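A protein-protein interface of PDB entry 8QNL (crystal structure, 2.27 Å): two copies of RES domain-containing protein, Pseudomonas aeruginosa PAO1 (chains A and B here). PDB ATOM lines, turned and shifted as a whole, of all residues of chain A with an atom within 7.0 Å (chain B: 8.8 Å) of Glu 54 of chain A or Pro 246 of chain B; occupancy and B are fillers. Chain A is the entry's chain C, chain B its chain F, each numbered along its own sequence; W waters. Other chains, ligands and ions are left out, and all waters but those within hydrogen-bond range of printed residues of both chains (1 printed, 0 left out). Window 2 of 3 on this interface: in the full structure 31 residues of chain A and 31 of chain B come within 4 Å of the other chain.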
ATOM      1  N   LEU A  47      21.453 -28.094  28.123  1.00  0.00           N
ATOM      2  CA  LEU A  47      20.330 -27.866  27.224  1.00  0.00           C
ATOM      3  C   LEU A  47      20.315 -28.880  26.083  1.00  0.00           C
ATOM      4  O   LEU A  47      19.247 -29.172  25.533  1.00  0.00           O
ATOM      5  CB  LEU A  47      20.375 -26.433  26.690  1.00  0.00           C
ATOM      6  CG  LEU A  47      19.163 -25.984  25.869  1.00  0.00           C
ATOM      7  CD1 LEU A  47      17.864 -26.266  26.616  1.00  0.00           C
ATOM      8  CD2 LEU A  47      19.268 -24.512  25.509  1.00  0.00           C
ATOM      9  N   VAL A  50      18.177 -32.201  27.266  1.00  0.00           N
ATOM     10  CA  VAL A  50      16.723 -32.185  27.406  1.00  0.00           C
ATOM     11  C   VAL A  50      16.106 -31.497  26.192  1.00  0.00           C
ATOM     12  O   VAL A  50      16.803 -31.192  25.218  1.00  0.00           O
ATOM     13  CB  VAL A  50      16.303 -31.500  28.719  1.00  0.00           C
ATOM     14  CG1 VAL A  50      16.799 -32.294  29.910  1.00  0.00           C
ATOM     15  CG2 VAL A  50      16.835 -30.084  28.772  1.00  0.00           C
ATOM     16  N   ASP A  51      14.797 -31.255  26.233  1.00  0.00           N
ATOM     17  CA  ASP A  51      14.105 -30.647  25.101  1.00  0.00           C
ATOM     18  C   ASP A  51      13.743 -29.186  25.313  1.00  0.00           C
ATOM     19  O   ASP A  51      13.858 -28.392  24.376  1.00  0.00           O
ATOM     20  CB  ASP A  51      12.837 -31.439  24.759  1.00  0.00           C
ATOM     21  CG  ASP A  51      13.135 -32.704  23.968  1.00  0.00           C
ATOM     22  OD1 ASP A  51      12.767 -33.807  24.428  1.00  0.00           O
ATOM     23  OD2 ASP A  51      13.760 -32.594  22.892  1.00  0.00           O
ATOM     24  N   THR A  52      13.330 -28.802  26.517  1.00  0.00           N
ATOM     25  CA  THR A  52      12.849 -27.455  26.782  1.00  0.00           C
ATOM     26  C   THR A  52      13.746 -26.749  27.790  1.00  0.00           C
ATOM     27  O   THR A  52      14.500 -27.378  28.538  1.00  0.00           O
ATOM     28  CB  THR A  52      11.400 -27.475  27.297  1.00  0.00           C
ATOM     29  OG1 THR A  52      11.360 -28.045  28.612  1.00  0.00           O
ATOM     30  CG2 THR A  52      10.523 -28.298  26.369  1.00  0.00           C
ATOM     31  N   LEU A  53      13.656 -25.415  27.794  1.00  0.00           N
ATOM     32  CA  LEU A  53      14.387 -24.626  28.777  1.00  0.00           C
ATOM     33  C   LEU A  53      13.883 -24.894  30.188  1.00  0.00           C
ATOM     34  O   LEU A  53      14.651 -24.796  31.152  1.00  0.00           O
ATOM     35  CB  LEU A  53      14.276 -23.138  28.448  1.00  0.00           C
ATOM     36  CG  LEU A  53      15.220 -22.587  27.382  1.00  0.00           C
ATOM     37  CD1 LEU A  53      15.015 -21.090  27.261  1.00  0.00           C
ATOM     38  CD2 LEU A  53      16.668 -22.909  27.730  1.00  0.00           C
ATOM     39  N   GLU A  54      12.598 -25.229  30.325  1.00  0.00           N
ATOM     40  CA  GLU A  54      12.061 -25.592  31.632  1.00  0.00           C
ATOM     41  C   GLU A  54      12.647 -26.909  32.131  1.00  0.00           C
ATOM     42  O   GLU A  54      12.940 -27.047  33.324  1.00  0.00           O
ATOM     43  CB  GLU A  54      10.536 -25.673  31.564  1.00  0.00           C
ATOM     44  CG  GLU A  54       9.887 -26.240  32.807  1.00  0.00           C
ATOM     45  CD  GLU A  54       9.710 -25.207  33.905  1.00  0.00           C
ATOM     46  OE1 GLU A  54      10.073 -24.031  33.691  1.00  0.00           O
ATOM     47  OE2 GLU A  54       9.197 -25.576  34.984  1.00  0.00           O
ATOM     48  N   GLU A  55      12.817 -27.892  31.240  1.00  0.00           N
ATOM     49  CA  GLU A  55      13.457 -29.141  31.644  1.00  0.00           C
ATOM     50  C   GLU A  55      14.916 -28.911  32.009  1.00  0.00           C
ATOM     51  O   GLU A  55      15.433 -29.520  32.954  1.00  0.00           O
ATOM     52  CB  GLU A  55      13.347 -30.186  30.531  1.00  0.00           C
ATOM     53  CG  GLU A  55      11.937 -30.730  30.291  1.00  0.00           C
ATOM     54  CD  GLU A  55      11.891 -31.753  29.161  1.00  0.00           C
ATOM     55  OE1 GLU A  55      12.954 -32.048  28.573  1.00  0.00           O
ATOM     56  OE2 GLU A  55      10.789 -32.259  28.858  1.00  0.00           O
ATOM     57  N   GLN A  56      15.597 -28.030  31.271  1.00  0.00           N
ATOM     58  CA  GLN A  56      16.989 -27.724  31.584  1.00  0.00           C
ATOM     59  C   GLN A  56      17.108 -27.014  32.928  1.00  0.00           C
ATOM     60  O   GLN A  56      18.035 -27.287  33.698  1.00  0.00           O
ATOM     61  CB  GLN A  56      17.598 -26.890  30.456  1.00  0.00           C
ATOM     62  CG  GLN A  56      19.103 -26.703  30.534  1.00  0.00           C
ATOM     63  CD  GLN A  56      19.480 -25.428  31.251  1.00  0.00           C
ATOM     64  OE1 GLN A  56      18.613 -24.672  31.679  1.00  0.00           O
ATOM     65  NE2 GLN A  56      20.779 -25.180  31.385  1.00  0.00           N
ATOM     66  N   ALA A  57      16.170 -26.113  33.238  1.00  0.00           N
ATOM     67  CA  ALA A  57      16.217 -25.427  34.525  1.00  0.00           C
ATOM     68  C   ALA A  57      16.030 -26.407  35.676  1.00  0.00           C
ATOM     69  O   ALA A  57      16.711 -26.304  36.704  1.00  0.00           O
ATOM     70  CB  ALA A  57      15.161 -24.325  34.579  1.00  0.00           C
ATOM     71  N   LEU A  58      15.123 -27.372  35.517  1.00  0.00           N
ATOM     72  CA  LEU A  58      14.942 -28.386  36.551  1.00  0.00           C
ATOM     73  C   LEU A  58      16.177 -29.272  36.674  1.00  0.00           C
ATOM     74  O   LEU A  58      16.589 -29.616  37.789  1.00  0.00           O
ATOM     75  CB  LEU A  58      13.699 -29.227  36.252  1.00  0.00           C
ATOM     76  CG  LEU A  58      13.408 -30.385  37.211  1.00  0.00           C
ATOM     77  CD1 LEU A  58      13.249 -29.884  38.641  1.00  0.00           C
ATOM     78  CD2 LEU A  58      12.165 -31.141  36.771  1.00  0.00           C
ATOM     79  N   LEU A  59      16.785 -29.645  35.545  1.00  0.00           N
ATOM     80  CA  LEU A  59      17.983 -30.480  35.591  1.00  0.00           C
ATOM     81  C   LEU A  59      19.131 -29.762  36.292  1.00  0.00           C
ATOM     82  O   LEU A  59      19.856 -30.368  37.089  1.00  0.00           O
ATOM     83  CB  LEU A  59      18.390 -30.896  34.177  1.00  0.00           C
ATOM     84  CG  LEU A  59      19.687 -31.703  34.062  1.00  0.00           C
ATOM     85  CD1 LEU A  59      19.553 -33.050  34.766  1.00  0.00           C
ATOM     86  CD2 LEU A  59      20.097 -31.886  32.606  1.00  0.00           C
ATOM     87  N   MET B 115      12.325  -8.394  26.092  1.00  0.00           N
ATOM     88  CA  MET B 115      12.113  -9.802  25.770  1.00  0.00           C
ATOM     89  C   MET B 115      10.833 -10.003  24.967  1.00  0.00           C
ATOM     90  O   MET B 115      10.782 -10.861  24.078  1.00  0.00           O
ATOM     91  CB  MET B 115      12.074 -10.643  27.044  1.00  0.00           C
ATOM     92  CG  MET B 115      13.421 -10.856  27.698  1.00  0.00           C
ATOM     93  SD  MET B 115      13.285 -12.045  29.048  1.00  0.00           S
ATOM     94  CE  MET B 115      12.248 -11.130  30.189  1.00  0.00           C
ATOM     95  N   ARG B 137      12.245 -26.683  16.894  1.00  0.00           N
ATOM     96  CA  ARG B 137      12.712 -25.937  18.058  1.00  0.00           C
ATOM     97  C   ARG B 137      14.080 -25.350  17.743  1.00  0.00           C
ATOM     98  O   ARG B 137      14.993 -26.080  17.346  1.00  0.00           O
ATOM     99  CB  ARG B 137      12.781 -26.839  19.298  1.00  0.00           C
ATOM    100  CG  ARG B 137      13.158 -26.113  20.581  1.00  0.00           C
ATOM    101  CD  ARG B 137      12.881 -26.966  21.817  1.00  0.00           C
ATOM    102  NE  ARG B 137      11.480 -26.937  22.243  1.00  0.00           N
ATOM    103  CZ  ARG B 137      10.622 -27.943  22.086  1.00  0.00           C
ATOM    104  NH1 ARG B 137      11.019 -29.072  21.513  1.00  0.00           N
ATOM    105  NH2 ARG B 137       9.368 -27.823  22.508  1.00  0.00           N
ATOM    106  N   TRP B 226      22.006 -14.807  27.234  1.00  0.00           N
ATOM    107  CA  TRP B 226      20.702 -15.439  27.370  1.00  0.00           C
ATOM    108  C   TRP B 226      20.610 -16.646  26.450  1.00  0.00           C
ATOM    109  O   TRP B 226      21.138 -16.630  25.334  1.00  0.00           O
ATOM    110  CB  TRP B 226      19.558 -14.460  27.050  1.00  0.00           C
ATOM    111  CG  TRP B 226      19.475 -13.305  27.992  1.00  0.00           C
ATOM    112  CD1 TRP B 226      20.153 -12.128  27.901  1.00  0.00           C
ATOM    113  CD2 TRP B 226      18.670 -13.215  29.174  1.00  0.00           C
ATOM    114  NE1 TRP B 226      19.825 -11.309  28.954  1.00  0.00           N
ATOM    115  CE2 TRP B 226      18.916 -11.953  29.750  1.00  0.00           C
ATOM    116  CE3 TRP B 226      17.768 -14.080  29.803  1.00  0.00           C
ATOM    117  CZ2 TRP B 226      18.290 -11.532  30.921  1.00  0.00           C
ATOM    118  CZ3 TRP B 226      17.149 -13.659  30.965  1.00  0.00           C
ATOM    119  CH2 TRP B 226      17.411 -12.398  31.512  1.00  0.00           C
ATOM    120  N   LEU B 227      19.945 -17.693  26.934  1.00  0.00           N
ATOM    121  CA  LEU B 227      19.560 -18.832  26.115  1.00  0.00           C
ATOM    122  C   LEU B 227      18.140 -18.609  25.613  1.00  0.00           C
ATOM    123  O   LEU B 227      17.255 -18.243  26.394  1.00  0.00           O
ATOM    124  CB  LEU B 227      19.652 -20.133  26.916  1.00  0.00           C
ATOM    125  CG  LEU B 227      21.032 -20.511  27.460  1.00  0.00           C
ATOM    126  CD1 LEU B 227      20.987 -21.858  28.170  1.00  0.00           C
ATOM    127  CD2 LEU B 227      22.061 -20.524  26.339  1.00  0.00           C
ATOM    128  N   CYS B 228      17.924 -18.819  24.315  1.00  0.00           N
ATOM    129  CA  CYS B 228      16.621 -18.618  23.696  1.00  0.00           C
ATOM    130  C   CYS B 228      16.122 -19.917  23.083  1.00  0.00           C
ATOM    131  O   CYS B 228      16.877 -20.638  22.421  1.00  0.00           O
ATOM    132  CB  CYS B 228      16.672 -17.534  22.617  1.00  0.00           C
ATOM    133  SG  CYS B 228      15.060 -17.203  21.832  1.00  0.00           S
ATOM    134  N   GLU B 229      14.843 -20.203  23.306  1.00  0.00           N
ATOM    135  CA  GLU B 229      14.180 -21.385  22.768  1.00  0.00           C
ATOM    136  C   GLU B 229      12.949 -20.916  22.004  1.00  0.00           C
ATOM    137  O   GLU B 229      12.013 -20.378  22.602  1.00  0.00           O
ATOM    138  CB  GLU B 229      13.796 -22.359  23.884  1.00  0.00           C
ATOM    139  CG  GLU B 229      13.009 -23.576  23.420  1.00  0.00           C
ATOM    140  CD  GLU B 229      12.373 -24.331  24.577  1.00  0.00           C
ATOM    141  OE1 GLU B 229      12.560 -23.911  25.739  1.00  0.00           O
ATOM    142  OE2 GLU B 229      11.682 -25.341  24.325  1.00  0.00           O
ATOM    143  N   TYR B 234       5.830 -21.134  21.442  1.00  0.00           N
ATOM    144  CA  TYR B 234       6.300 -20.180  22.439  1.00  0.00           C
ATOM    145  C   TYR B 234       7.745 -19.799  22.164  1.00  0.00           C
ATOM    146  O   TYR B 234       8.451 -20.445  21.388  1.00  0.00           O
ATOM    147  CB  TYR B 234       6.173 -20.741  23.857  1.00  0.00           C
ATOM    148  CG  TYR B 234       7.043 -21.951  24.127  1.00  0.00           C
ATOM    149  CD1 TYR B 234       6.598 -23.228  23.821  1.00  0.00           C
ATOM    150  CD2 TYR B 234       8.307 -21.815  24.696  1.00  0.00           C
ATOM    151  CE1 TYR B 234       7.382 -24.338  24.064  1.00  0.00           C
ATOM    152  CE2 TYR B 234       9.100 -22.924  24.944  1.00  0.00           C
ATOM    153  CZ  TYR B 234       8.630 -24.183  24.628  1.00  0.00           C
ATOM    154  OH  TYR B 234       9.405 -25.293  24.871  1.00  0.00           O
ATOM    155  N   VAL B 235       8.174 -18.740  22.841  1.00  0.00           N
ATOM    156  CA  VAL B 235       9.564 -18.312  22.879  1.00  0.00           C
ATOM    157  C   VAL B 235       9.961 -18.177  24.340  1.00  0.00           C
ATOM    158  O   VAL B 235       9.264 -17.513  25.115  1.00  0.00           O
ATOM    159  CB  VAL B 235       9.776 -16.982  22.132  1.00  0.00           C
ATOM    160  CG1 VAL B 235      11.221 -16.526  22.260  1.00  0.00           C
ATOM    161  CG2 VAL B 235       9.372 -17.123  20.665  1.00  0.00           C
ATOM    162  N   ALA B 236      11.069 -18.810  24.721  1.00  0.00           N
ATOM    163  CA  ALA B 236      11.516 -18.815  26.106  1.00  0.00           C
ATOM    164  C   ALA B 236      12.946 -18.303  26.201  1.00  0.00           C
ATOM    165  O   ALA B 236      13.794 -18.637  25.366  1.00  0.00           O
ATOM    166  CB  ALA B 236      11.418 -20.219  26.714  1.00  0.00           C
ATOM    167  N   PHE B 237      13.205 -17.490  27.223  1.00  0.00           N
ATOM    168  CA  PHE B 237      14.522 -16.921  27.479  1.00  0.00           C
ATOM    169  C   PHE B 237      14.990 -17.321  28.870  1.00  0.00           C
ATOM    170  O   PHE B 237      14.193 -17.381  29.811  1.00  0.00           O
ATOM    171  CB  PHE B 237      14.513 -15.392  27.371  1.00  0.00           C
ATOM    172  CG  PHE B 237      14.141 -14.872  26.012  1.00  0.00           C
ATOM    173  CD1 PHE B 237      15.082 -14.807  24.998  1.00  0.00           C
ATOM    174  CD2 PHE B 237      12.854 -14.426  25.757  1.00  0.00           C
ATOM    175  CE1 PHE B 237      14.743 -14.317  23.748  1.00  0.00           C
ATOM    176  CE2 PHE B 237      12.509 -13.935  24.511  1.00  0.00           C
ATOM    177  CZ  PHE B 237      13.455 -13.882  23.505  1.00  0.00           C
ATOM    178  N   LYS B 238      16.295 -17.574  28.997  1.00  0.00           N
ATOM    179  CA  LYS B 238      16.890 -17.960  30.265  1.00  0.00           C
ATOM    180  C   LYS B 238      18.331 -17.469  30.303  1.00  0.00           C
ATOM    181  O   LYS B 238      19.031 -17.554  29.282  1.00  0.00           O
ATOM    182  CB  LYS B 238      16.852 -19.481  30.469  1.00  0.00           C
ATOM    183  CG  LYS B 238      17.401 -19.922  31.805  1.00  0.00           C
ATOM    184  CD  LYS B 238      17.562 -21.424  31.914  1.00  0.00           C
ATOM    185  CE  LYS B 238      18.418 -21.757  33.128  1.00  0.00           C
ATOM    186  NZ  LYS B 238      18.493 -23.213  33.411  1.00  0.00           N
ATOM    187  N   PRO B 239      18.797 -16.947  31.438  1.00  0.00           N
ATOM    188  CA  PRO B 239      20.211 -16.561  31.539  1.00  0.00           C
ATOM    189  C   PRO B 239      21.125 -17.735  31.215  1.00  0.00           C
ATOM    190  O   PRO B 239      20.870 -18.875  31.615  1.00  0.00           O
ATOM    191  CB  PRO B 239      20.355 -16.115  32.999  1.00  0.00           C
ATOM    192  CG  PRO B 239      18.974 -15.666  33.384  1.00  0.00           C
ATOM    193  CD  PRO B 239      18.033 -16.584  32.646  1.00  0.00           C
ATOM    194  N   PRO B 243      22.214 -19.543  37.345  1.00  0.00           N
ATOM    195  CA  PRO B 243      21.034 -20.355  37.494  1.00  0.00           C
ATOM    196  C   PRO B 243      19.782 -19.477  37.431  1.00  0.00           C
ATOM    197  O   PRO B 243      19.797 -18.402  37.954  1.00  0.00           O
ATOM    198  CB  PRO B 243      21.214 -20.980  38.882  1.00  0.00           C
ATOM    199  CG  PRO B 243      22.685 -20.960  39.109  1.00  0.00           C
ATOM    200  CD  PRO B 243      23.028 -19.595  38.582  1.00  0.00           C
ATOM    201  N   GLY B 244      18.734 -19.983  36.796  1.00  0.00           N
ATOM    202  CA  GLY B 244      17.485 -19.226  36.683  1.00  0.00           C
ATOM    203  C   GLY B 244      16.377 -20.033  36.058  1.00  0.00           C
ATOM    204  O   GLY B 244      16.647 -21.142  35.611  1.00  0.00           O
ATOM    205  N   SER B 245      15.170 -19.489  36.067  1.00  0.00           N
ATOM    206  CA  SER B 245      13.994 -20.168  35.480  1.00  0.00           C
ATOM    207  C   SER B 245      13.619 -19.459  34.182  1.00  0.00           C
ATOM    208  O   SER B 245      13.759 -18.242  34.130  1.00  0.00           O
ATOM    209  CB  SER B 245      12.855 -20.144  36.438  1.00  0.00           C
ATOM    210  OG  SER B 245      12.063 -18.984  36.247  1.00  0.00           O
ATOM    211  N   PRO B 246      13.153 -20.164  33.138  1.00  0.00           N
ATOM    212  CA  PRO B 246      12.892 -19.493  31.858  1.00  0.00           C
ATOM    213  C   PRO B 246      11.717 -18.531  31.944  1.00  0.00           C
ATOM    214  O   PRO B 246      10.725 -18.786  32.630  1.00  0.00           O
ATOM    215  CB  PRO B 246      12.594 -20.655  30.903  1.00  0.00           C
ATOM    216  CG  PRO B 246      12.089 -21.741  31.789  1.00  0.00           C
ATOM    217  CD  PRO B 246      12.854 -21.605  33.077  1.00  0.00           C
ATOM    218  N   LYS B 247      11.845 -17.411  31.241  1.00  0.00           N
ATOM    219  CA  LYS B 247      10.748 -16.474  31.036  1.00  0.00           C
ATOM    220  C   LYS B 247      10.118 -16.808  29.690  1.00  0.00           C
ATOM    221  O   LYS B 247      10.751 -16.634  28.643  1.00  0.00           O
ATOM    222  CB  LYS B 247      11.249 -15.032  31.081  1.00  0.00           C
ATOM    223  CG  LYS B 247      10.147 -13.984  31.119  1.00  0.00           C
ATOM    224  CD  LYS B 247       9.782 -13.603  32.548  1.00  0.00           C
ATOM    225  CE  LYS B 247       8.672 -12.562  32.573  1.00  0.00           C
ATOM    226  NZ  LYS B 247       7.402 -13.093  32.001  1.00  0.00           N
ATOM    227  N   ILE B 248       8.880 -17.300  29.713  1.00  0.00           N
ATOM    228  CA  ILE B 248       8.231 -17.851  28.526  1.00  0.00           C
ATOM    229  C   ILE B 248       7.249 -16.836  27.959  1.00  0.00           C
ATOM    230  O   ILE B 248       6.505 -16.181  28.703  1.00  0.00           O
ATOM    231  CB  ILE B 248       7.527 -19.184  28.848  1.00  0.00           C
ATOM    232  CG1 ILE B 248       8.405 -20.037  29.768  1.00  0.00           C
ATOM    233  CG2 ILE B 248       7.218 -19.945  27.564  1.00  0.00           C
ATOM    234  CD1 ILE B 248       7.816 -21.389  30.113  1.00  0.00           C
ATOM    235  N   PHE B 249       7.246 -16.708  26.633  1.00  0.00           N
ATOM    236  CA  PHE B 249       6.356 -15.811  25.898  1.00  0.00           C
ATOM    237  C   PHE B 249       5.601 -16.644  24.866  1.00  0.00           C
ATOM    238  O   PHE B 249       6.163 -17.023  23.834  1.00  0.00           O
ATOM    239  CB  PHE B 249       7.138 -14.679  25.232  1.00  0.00           C
ATOM    240  CG  PHE B 249       7.725 -13.696  26.199  1.00  0.00           C
ATOM    241  CD1 PHE B 249       8.923 -13.966  26.839  1.00  0.00           C
ATOM    242  CD2 PHE B 249       7.081 -12.501  26.469  1.00  0.00           C
ATOM    243  CE1 PHE B 249       9.466 -13.063  27.734  1.00  0.00           C
ATOM    244  CE2 PHE B 249       7.618 -11.594  27.362  1.00  0.00           C
ATOM    245  CZ  PHE B 249       8.812 -11.876  27.996  1.00  0.00           C
HETATM  246  O   HOH W   1      10.869 -24.249  27.769  1.00  0.00           O
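No position is printed for both chains.
CD of Arg 137 of chain B touches O of Asp 51 of chain A, 3.1 Å away.
Asp 51 of chain A touches Glu 229 of chain B (O to OE2, 3.7 Å).
CA of Thr 52 of chain A touches OE2 of Glu 229 of chain B (3.4 Å).
Thr 52 of chain A touches Tyr 234 of chain B (CG2 to OH, 3.5 Å).
Leu 227 of chain B touches Leu 53 of chain A.
Leu 53 of chain A touches Ala 236 of chain B (CD1 to O, 3.3 Å).
Pro 246 of chain B touches Leu 53 of chain A.
Glu 54 of chain A touches Pro 246 of chain B.
Lys 238 of chain B touches Ala 57 of chain A.
Ala 57 of chain A touches Gly 244 of chain B.
The backbone NH of Leu 53 of chain A sits at hydrogen-bond distance from the side-chain carboxylate of Glu 229 of chain B, 2.8 Å away.
The side-chain amide oxygen (OE1) of Gln 56 of chain A sits close to the side-chain amino group (NZ) of Lys 238 of chain B (2.3 Å).
The side-chain carboxylate (OE1) of Glu 55 of chain A sits at hydrogen-bond distance from the backbone NH (N) of Asp 51 of chain A (3.1 Å).
N of Glu 55 of chain A is in hydrogen-bond range of OG1 of Thr 52 of chain A (3.0 Å).
The guanidinium group (NE) of Arg 137 of chain B lies within salt-bridge range of the side-chain carboxylate (OE2) of Glu 229 of chain B (2.6 Å).
The guanidinium group (NH2) of Arg 137 of chain B sits at hydrogen-bond distance from the side-chain hydroxyl (OH) of Tyr 234 of chain B, 3.5 Å away.
The backbone carbonyl oxygen of Lys 238 of chain B sits at hydrogen-bond distance from the backbone NH of Leu 227 of chain B (2.5 Å).
The backbone NH (N) of Glu 229 of chain B is in hydrogen-bond range of the backbone carbonyl oxygen (O) of Ala 236 of chain B (2.8 Å).
Water W1 lies within hydrogen-bond range of OE1 of Glu 229 of chain B (2.7 Å), N of Leu 53 of chain A (3.0 Å), N of Glu 54 of chain A (3.2 Å) and OH of Tyr 234 of chain B (3.4 Å).
Printed residues of chain B within 4 Å of Glu 54 of chain A: Pro 246 (3.6 Å).
Of the printed residues of chain A, Pro 246 of chain B touches Leu 53 (3.9 Å), Glu 54 (3.6 Å) and Ala 57 (3.9 Å).
Of the printed residues of chain A, Lys 238 of chain B touches Gln 56 (2.3 Å) and Ala 57 (3.4 Å).
Of the printed residues of chain A, Leu 227 of chain B touches Leu 53.
Of the printed residues of chain B, Thr 52 of chain A touches Glu 229 (3.4 Å) and Tyr 234 (3.5 Å).
Of the printed residues of chain B, Gln 56 of chain A touches Lys 238 (2.3 Å).
Phe 237 of chain B touches none of the printed residues of chain A.
Of the 19 printed residues of chain B, 8 touch a printed residue of chain A.
Printed residues of chain B that touch a printed residue of chain A: Arg 137, Leu 227, Glu 229, Tyr 234, Ala 236, Lys 238, Gly 244 and Pro 246.
Hydrophobic or aromatic side chains of chain B that line the printed part of chain A: Tyr 234, Ala 236 and Pro 246.
Along chain B the printed residues that touch a printed residue of chain A span positions 137 to 246.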
